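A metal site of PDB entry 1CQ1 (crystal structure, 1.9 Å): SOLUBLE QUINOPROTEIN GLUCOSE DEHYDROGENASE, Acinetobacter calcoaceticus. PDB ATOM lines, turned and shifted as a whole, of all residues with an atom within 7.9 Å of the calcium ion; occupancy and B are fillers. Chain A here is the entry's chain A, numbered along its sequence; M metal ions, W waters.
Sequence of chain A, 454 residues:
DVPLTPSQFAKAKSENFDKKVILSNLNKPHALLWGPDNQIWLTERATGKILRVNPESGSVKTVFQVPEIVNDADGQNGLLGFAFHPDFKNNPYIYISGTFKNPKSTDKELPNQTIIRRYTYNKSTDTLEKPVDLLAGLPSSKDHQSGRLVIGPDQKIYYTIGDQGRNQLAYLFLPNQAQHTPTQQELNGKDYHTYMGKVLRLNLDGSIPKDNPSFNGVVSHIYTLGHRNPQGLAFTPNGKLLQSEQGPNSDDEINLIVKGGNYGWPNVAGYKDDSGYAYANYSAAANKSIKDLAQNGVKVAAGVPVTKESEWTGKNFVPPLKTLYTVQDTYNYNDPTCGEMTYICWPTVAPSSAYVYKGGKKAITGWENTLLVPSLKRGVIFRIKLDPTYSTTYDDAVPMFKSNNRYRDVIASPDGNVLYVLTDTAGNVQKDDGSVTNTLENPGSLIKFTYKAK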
ATOM      1  N   SER A 250      26.764  30.488 -10.876  1.00  0.00           N
ATOM      2  CA  SER A 250      25.709  30.057 -11.783  1.00  0.00           C
ATOM      3  C   SER A 250      24.642  29.288 -11.022  1.00  0.00           C
ATOM      4  O   SER A 250      24.817  28.955  -9.855  1.00  0.00           O
ATOM      5  CB  SER A 250      26.305  29.117 -12.860  1.00  0.00           C
ATOM      6  OG  SER A 250      26.775  27.938 -12.221  1.00  0.00           O
ATOM      7  N   ASP A 251      23.668  28.814 -11.792  1.00  0.00           N
ATOM      8  CA  ASP A 251      22.740  27.803 -11.299  1.00  0.00           C
ATOM      9  C   ASP A 251      21.989  28.187 -10.035  1.00  0.00           C
ATOM     10  O   ASP A 251      21.926  27.402  -9.089  1.00  0.00           O
ATOM     11  CB  ASP A 251      23.507  26.480 -11.086  1.00  0.00           C
ATOM     12  CG  ASP A 251      23.916  25.873 -12.432  1.00  0.00           C
ATOM     13  OD1 ASP A 251      22.998  25.397 -13.128  1.00  0.00           O
ATOM     14  OD2 ASP A 251      25.117  25.893 -12.770  1.00  0.00           O
ATOM     15  N   GLU A 253      18.489  28.245  -8.285  1.00  0.00           N
ATOM     16  CA  GLU A 253      17.506  27.202  -8.508  1.00  0.00           C
ATOM     17  C   GLU A 253      16.089  27.535  -8.072  1.00  0.00           C
ATOM     18  O   GLU A 253      15.851  28.229  -7.076  1.00  0.00           O
ATOM     19  CB  GLU A 253      17.898  25.940  -7.703  1.00  0.00           C
ATOM     20  CG  GLU A 253      19.239  25.353  -8.080  1.00  0.00           C
ATOM     21  CD  GLU A 253      19.605  24.113  -7.314  1.00  0.00           C
ATOM     22  OE1 GLU A 253      19.001  23.783  -6.272  1.00  0.00           O
ATOM     23  OE2 GLU A 253      20.548  23.400  -7.742  1.00  0.00           O
ATOM     24  N   ASN A 267      28.322  19.463  -3.983  1.00  0.00           N
ATOM     25  CA  ASN A 267      28.875  18.621  -5.063  1.00  0.00           C
ATOM     26  C   ASN A 267      28.213  18.881  -6.399  1.00  0.00           C
ATOM     27  O   ASN A 267      28.844  18.705  -7.450  1.00  0.00           O
ATOM     28  CB  ASN A 267      28.716  17.156  -4.670  1.00  0.00           C
ATOM     29  CG  ASN A 267      29.570  16.803  -3.457  1.00  0.00           C
ATOM     30  OD1 ASN A 267      30.700  16.349  -3.634  1.00  0.00           O
ATOM     31  ND2 ASN A 267      29.024  16.977  -2.271  1.00  0.00           N
ATOM     32  N   VAL A 268      26.966  19.376  -6.370  1.00  0.00           N
ATOM     33  CA  VAL A 268      26.257  19.667  -7.599  1.00  0.00           C
ATOM     34  C   VAL A 268      25.510  20.994  -7.539  1.00  0.00           C
ATOM     35  O   VAL A 268      24.671  21.219  -6.683  1.00  0.00           O
ATOM     36  CB  VAL A 268      25.241  18.564  -7.950  1.00  0.00           C
ATOM     37  CG1 VAL A 268      24.580  18.832  -9.296  1.00  0.00           C
ATOM     38  CG2 VAL A 268      25.920  17.191  -7.951  1.00  0.00           C
ATOM     39  N   ALA A 269      25.740  21.840  -8.524  1.00  0.00           N
ATOM     40  CA  ALA A 269      25.083  23.113  -8.717  1.00  0.00           C
ATOM     41  C   ALA A 269      24.060  22.998  -9.846  1.00  0.00           C
ATOM     42  O   ALA A 269      24.493  22.837 -10.991  1.00  0.00           O
ATOM     43  CB  ALA A 269      26.101  24.198  -9.104  1.00  0.00           C
ATOM     44  N   GLY A 270      22.780  23.159  -9.574  1.00  0.00           N
ATOM     45  CA  GLY A 270      21.767  23.004 -10.625  1.00  0.00           C
ATOM     46  C   GLY A 270      21.668  21.529 -11.014  1.00  0.00           C
ATOM     47  O   GLY A 270      21.583  20.633 -10.183  1.00  0.00           O
ATOM     48  N   TYR A 271      21.578  21.285 -12.329  1.00  0.00           N
ATOM     49  CA  TYR A 271      21.515  19.906 -12.820  1.00  0.00           C
ATOM     50  C   TYR A 271      22.828  19.166 -12.643  1.00  0.00           C
ATOM     51  O   TYR A 271      23.894  19.778 -12.630  1.00  0.00           O
ATOM     52  CB  TYR A 271      21.175  19.902 -14.319  1.00  0.00           C
ATOM     53  CG  TYR A 271      19.882  20.624 -14.631  1.00  0.00           C
ATOM     54  CD1 TYR A 271      19.901  21.892 -15.199  1.00  0.00           C
ATOM     55  CD2 TYR A 271      18.661  20.038 -14.337  1.00  0.00           C
ATOM     56  CE1 TYR A 271      18.724  22.558 -15.485  1.00  0.00           C
ATOM     57  CE2 TYR A 271      17.471  20.712 -14.616  1.00  0.00           C
ATOM     58  CZ  TYR A 271      17.516  21.955 -15.186  1.00  0.00           C
ATOM     59  OH  TYR A 271      16.347  22.632 -15.472  1.00  0.00           O
ATOM     60  N   LYS A 272      22.758  17.832 -12.551  1.00  0.00           N
ATOM     61  CA  LYS A 272      23.991  17.055 -12.494  1.00  0.00           C
ATOM     62  C   LYS A 272      24.458  16.935 -13.953  1.00  0.00           C
ATOM     63  O   LYS A 272      24.160  15.930 -14.617  1.00  0.00           O
ATOM     64  CB  LYS A 272      23.824  15.692 -11.848  1.00  0.00           C
ATOM     65  CG  LYS A 272      25.169  15.009 -11.602  1.00  0.00           C
ATOM     66  CD  LYS A 272      24.997  13.562 -11.214  1.00  0.00           C
ATOM     67  CE  LYS A 272      24.313  13.326  -9.874  1.00  0.00           C
ATOM     68  NZ  LYS A 272      24.297  11.880  -9.530  1.00  0.00           N
ATOM     69  N   ASP A 273      25.098  17.988 -14.457  1.00  0.00           N
ATOM     70  CA  ASP A 273      25.415  18.052 -15.874  1.00  0.00           C
ATOM     71  C   ASP A 273      26.883  18.326 -16.193  1.00  0.00           C
ATOM     72  O   ASP A 273      27.204  18.460 -17.383  1.00  0.00           O
ATOM     73  CB  ASP A 273      24.517  19.112 -16.540  1.00  0.00           C
ATOM     74  CG  ASP A 273      24.679  20.485 -15.880  1.00  0.00           C
ATOM     75  OD1 ASP A 273      25.601  20.646 -15.062  1.00  0.00           O
ATOM     76  OD2 ASP A 273      23.904  21.403 -16.187  1.00  0.00           O
ATOM     77  N   ASP A 274      27.714  18.521 -15.175  1.00  0.00           N
ATOM     78  CA  ASP A 274      29.115  18.855 -15.374  1.00  0.00           C
ATOM     79  C   ASP A 274      29.306  20.027 -16.336  1.00  0.00           C
ATOM     80  O   ASP A 274      30.270  20.068 -17.098  1.00  0.00           O
ATOM     81  CB  ASP A 274      29.924  17.668 -15.913  1.00  0.00           C
ATOM     82  CG  ASP A 274      30.183  16.522 -15.001  1.00  0.00           C
ATOM     83  OD1 ASP A 274      29.835  16.500 -13.802  1.00  0.00           O
ATOM     84  OD2 ASP A 274      30.801  15.537 -15.485  1.00  0.00           O
ATOM     85  N   SER A 275      28.398  20.993 -16.286  1.00  0.00           N
ATOM     86  CA  SER A 275      28.452  22.154 -17.165  1.00  0.00           C
ATOM     87  C   SER A 275      28.567  23.471 -16.389  1.00  0.00           C
ATOM     88  O   SER A 275      27.600  23.872 -15.745  1.00  0.00           O
ATOM     89  CB  SER A 275      27.174  22.160 -17.996  1.00  0.00           C
ATOM     90  OG  SER A 275      27.183  23.175 -18.992  1.00  0.00           O
ATOM     91  N   GLY A 276      29.715  24.140 -16.497  1.00  0.00           N
ATOM     92  CA  GLY A 276      29.901  25.452 -15.906  1.00  0.00           C
ATOM     93  C   GLY A 276      30.245  25.515 -14.431  1.00  0.00           C
ATOM     94  O   GLY A 276      30.445  26.627 -13.915  1.00  0.00           O
ATOM     95  N   TYR A 277      30.302  24.399 -13.739  1.00  0.00           N
ATOM     96  CA  TYR A 277      30.620  24.290 -12.336  1.00  0.00           C
ATOM     97  C   TYR A 277      31.329  22.966 -12.072  1.00  0.00           C
ATOM     98  O   TYR A 277      31.105  21.985 -12.785  1.00  0.00           O
ATOM     99  CB  TYR A 277      29.343  24.341 -11.471  1.00  0.00           C
ATOM    100  CG  TYR A 277      29.574  24.120  -9.992  1.00  0.00           C
ATOM    101  CD1 TYR A 277      29.987  25.168  -9.155  1.00  0.00           C
ATOM    102  CD2 TYR A 277      29.387  22.872  -9.419  1.00  0.00           C
ATOM    103  CE1 TYR A 277      30.205  24.951  -7.804  1.00  0.00           C
ATOM    104  CE2 TYR A 277      29.606  22.656  -8.067  1.00  0.00           C
ATOM    105  CZ  TYR A 277      30.027  23.717  -7.263  1.00  0.00           C
ATOM    106  OH  TYR A 277      30.229  23.470  -5.921  1.00  0.00           O
ATOM    107  N   ALA A 278      32.167  22.951 -11.055  1.00  0.00           N
ATOM    108  CA  ALA A 278      32.792  21.753 -10.514  1.00  0.00           C
ATOM    109  C   ALA A 278      33.082  22.043  -9.037  1.00  0.00           C
ATOM    110  O   ALA A 278      33.189  23.232  -8.683  1.00  0.00           O
ATOM    111  CB  ALA A 278      34.020  21.332 -11.278  1.00  0.00           C
ATOM    112  N   GLU A 309      30.611  17.033 -11.057  1.00  0.00           N
ATOM    113  CA  GLU A 309      29.259  16.701 -10.586  1.00  0.00           C
ATOM    114  C   GLU A 309      28.967  15.222 -10.816  1.00  0.00           C
ATOM    115  O   GLU A 309      28.434  14.501  -9.969  1.00  0.00           O
ATOM    116  CB  GLU A 309      28.236  17.593 -11.291  1.00  0.00           C
ATOM    117  CG  GLU A 309      28.414  19.076 -11.010  1.00  0.00           C
ATOM    118  CD  GLU A 309      27.398  19.954 -11.699  1.00  0.00           C
ATOM    119  OE1 GLU A 309      27.051  19.692 -12.879  1.00  0.00           O
ATOM    120  OE2 GLU A 309      26.935  20.932 -11.081  1.00  0.00           O
ATOM    121  N   PHE A 317      19.493  12.346  -4.781  1.00  0.00           N
ATOM    122  CA  PHE A 317      19.670  13.643  -5.426  1.00  0.00           C
ATOM    123  C   PHE A 317      18.427  14.040  -6.212  1.00  0.00           C
ATOM    124  O   PHE A 317      17.973  13.308  -7.091  1.00  0.00           O
ATOM    125  CB  PHE A 317      20.881  13.653  -6.373  1.00  0.00           C
ATOM    126  CG  PHE A 317      20.957  14.930  -7.172  1.00  0.00           C
ATOM    127  CD1 PHE A 317      21.164  16.143  -6.514  1.00  0.00           C
ATOM    128  CD2 PHE A 317      20.809  14.937  -8.546  1.00  0.00           C
ATOM    129  CE1 PHE A 317      21.225  17.318  -7.223  1.00  0.00           C
ATOM    130  CE2 PHE A 317      20.872  16.129  -9.260  1.00  0.00           C
ATOM    131  CZ  PHE A 317      21.069  17.322  -8.592  1.00  0.00           C
ATOM    132  N   PRO A 320      16.819  20.567  -9.733  1.00  0.00           N
ATOM    133  CA  PRO A 320      15.940  21.733  -9.735  1.00  0.00           C
ATOM    134  C   PRO A 320      14.870  21.664 -10.820  1.00  0.00           C
ATOM    135  O   PRO A 320      15.139  21.101 -11.897  1.00  0.00           O
ATOM    136  CB  PRO A 320      16.912  22.874 -10.014  1.00  0.00           C
ATOM    137  CG  PRO A 320      18.018  22.238 -10.810  1.00  0.00           C
ATOM    138  CD  PRO A 320      18.198  20.874 -10.207  1.00  0.00           C
ATOM    139  N   THR A 323      16.773  26.433 -13.532  1.00  0.00           N
ATOM    140  CA  THR A 323      18.048  27.021 -13.137  1.00  0.00           C
ATOM    141  C   THR A 323      18.147  28.424 -13.715  1.00  0.00           C
ATOM    142  O   THR A 323      17.746  28.684 -14.856  1.00  0.00           O
ATOM    143  CB  THR A 323      19.275  26.219 -13.592  1.00  0.00           C
ATOM    144  OG1 THR A 323      19.234  26.055 -15.020  1.00  0.00           O
ATOM    145  CG2 THR A 323      19.327  24.864 -12.897  1.00  0.00           C
ATOM    146  N   TYR A 325      21.270  30.781 -13.777  1.00  0.00           N
ATOM    147  CA  TYR A 325      21.103  30.060 -15.017  1.00  0.00           C
ATOM    148  C   TYR A 325      22.166  28.986 -15.232  1.00  0.00           C
ATOM    149  O   TYR A 325      23.165  28.916 -14.519  1.00  0.00           O
ATOM    150  CB  TYR A 325      21.230  31.037 -16.195  1.00  0.00           C
ATOM    151  CG  TYR A 325      20.243  32.174 -16.201  1.00  0.00           C
ATOM    152  CD1 TYR A 325      20.568  33.436 -15.734  1.00  0.00           C
ATOM    153  CD2 TYR A 325      18.955  31.973 -16.679  1.00  0.00           C
ATOM    154  CE1 TYR A 325      19.637  34.468 -15.760  1.00  0.00           C
ATOM    155  CE2 TYR A 325      18.016  32.993 -16.706  1.00  0.00           C
ATOM    156  CZ  TYR A 325      18.374  34.239 -16.223  1.00  0.00           C
ATOM    157  OH  TYR A 325      17.435  35.252 -16.256  1.00  0.00           O
ATOM    158  N   THR A 326      21.987  28.206 -16.310  1.00  0.00           N
ATOM    159  CA  THR A 326      22.998  27.184 -16.612  1.00  0.00           C
ATOM    160  C   THR A 326      23.822  27.604 -17.824  1.00  0.00           C
ATOM    161  O   THR A 326      23.264  28.144 -18.786  1.00  0.00           O
ATOM    162  CB  THR A 326      22.387  25.795 -16.844  1.00  0.00           C
ATOM    163  OG1 THR A 326      21.664  25.404 -15.675  1.00  0.00           O
ATOM    164  CG2 THR A 326      23.498  24.788 -17.110  1.00  0.00           C
ATOM    165  N   VAL A 327      25.144  27.452 -17.753  1.00  0.00           N
ATOM    166  CA  VAL A 327      26.006  27.820 -18.876  1.00  0.00           C
ATOM    167  C   VAL A 327      26.995  26.692 -19.159  1.00  0.00           C
ATOM    168  O   VAL A 327      27.093  25.761 -18.363  1.00  0.00           O
ATOM    169  CB  VAL A 327      26.823  29.109 -18.604  1.00  0.00           C
ATOM    170  CG1 VAL A 327      25.902  30.293 -18.408  1.00  0.00           C
ATOM    171  CG2 VAL A 327      27.744  28.900 -17.412  1.00  0.00           C
HETATM  172 CA    CA M   1      25.367  21.565 -12.829  1.00  0.00          CA
HETATM  173  O   HOH W   1      23.579  22.726 -13.943  1.00  0.00           O
HETATM  174  O   HOH W   2      26.553  23.594 -13.243  1.00  0.00           O
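Water W1 lies within hydrogen-bond range of the side-chain carboxylate (OD2) of Asp 273 (2.6 Å), the side-chain carboxylate (OD1) of Asp 251 (2.9 Å) and the backbone NH (N) of Tyr 271 (2.9 Å).
Water W2 bridges the backbone carbonyl oxygen of Ser 275 (2.7 Å) and the side-chain carboxylate of Asp 251 (2.8 Å).
The side-chain carboxylate of Asp 273 sits close to the backbone NH of Ser 275, 3.1 Å away.
The side-chain carboxylate of Asp 274 sits at hydrogen-bond distance from the backbone NH of Glu 309.
O of Tyr 271 is bound to the calcium ion.
The calcium ion is bound by water W2, 2.4 Å away.
The calcium ion is bound by O of Ala 269.
Water W1 binds the calcium ion.
The side-chain carboxylate (OD1) of Asp 273 binds the calcium ion, 2.4 Å away.
OE2 of Glu 309 binds the calcium ion (2.4 Å).
OE1 of Glu 309 is bound to the calcium ion.
The calcium ion has seven donor atoms within binding distance.
Within 4 Å of the calcium ion: Ala 269, Tyr 271, Asp 273 and Glu 309.
The nearest printed residue that does not touch the calcium ion is Gly 270 (4.1 Å).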
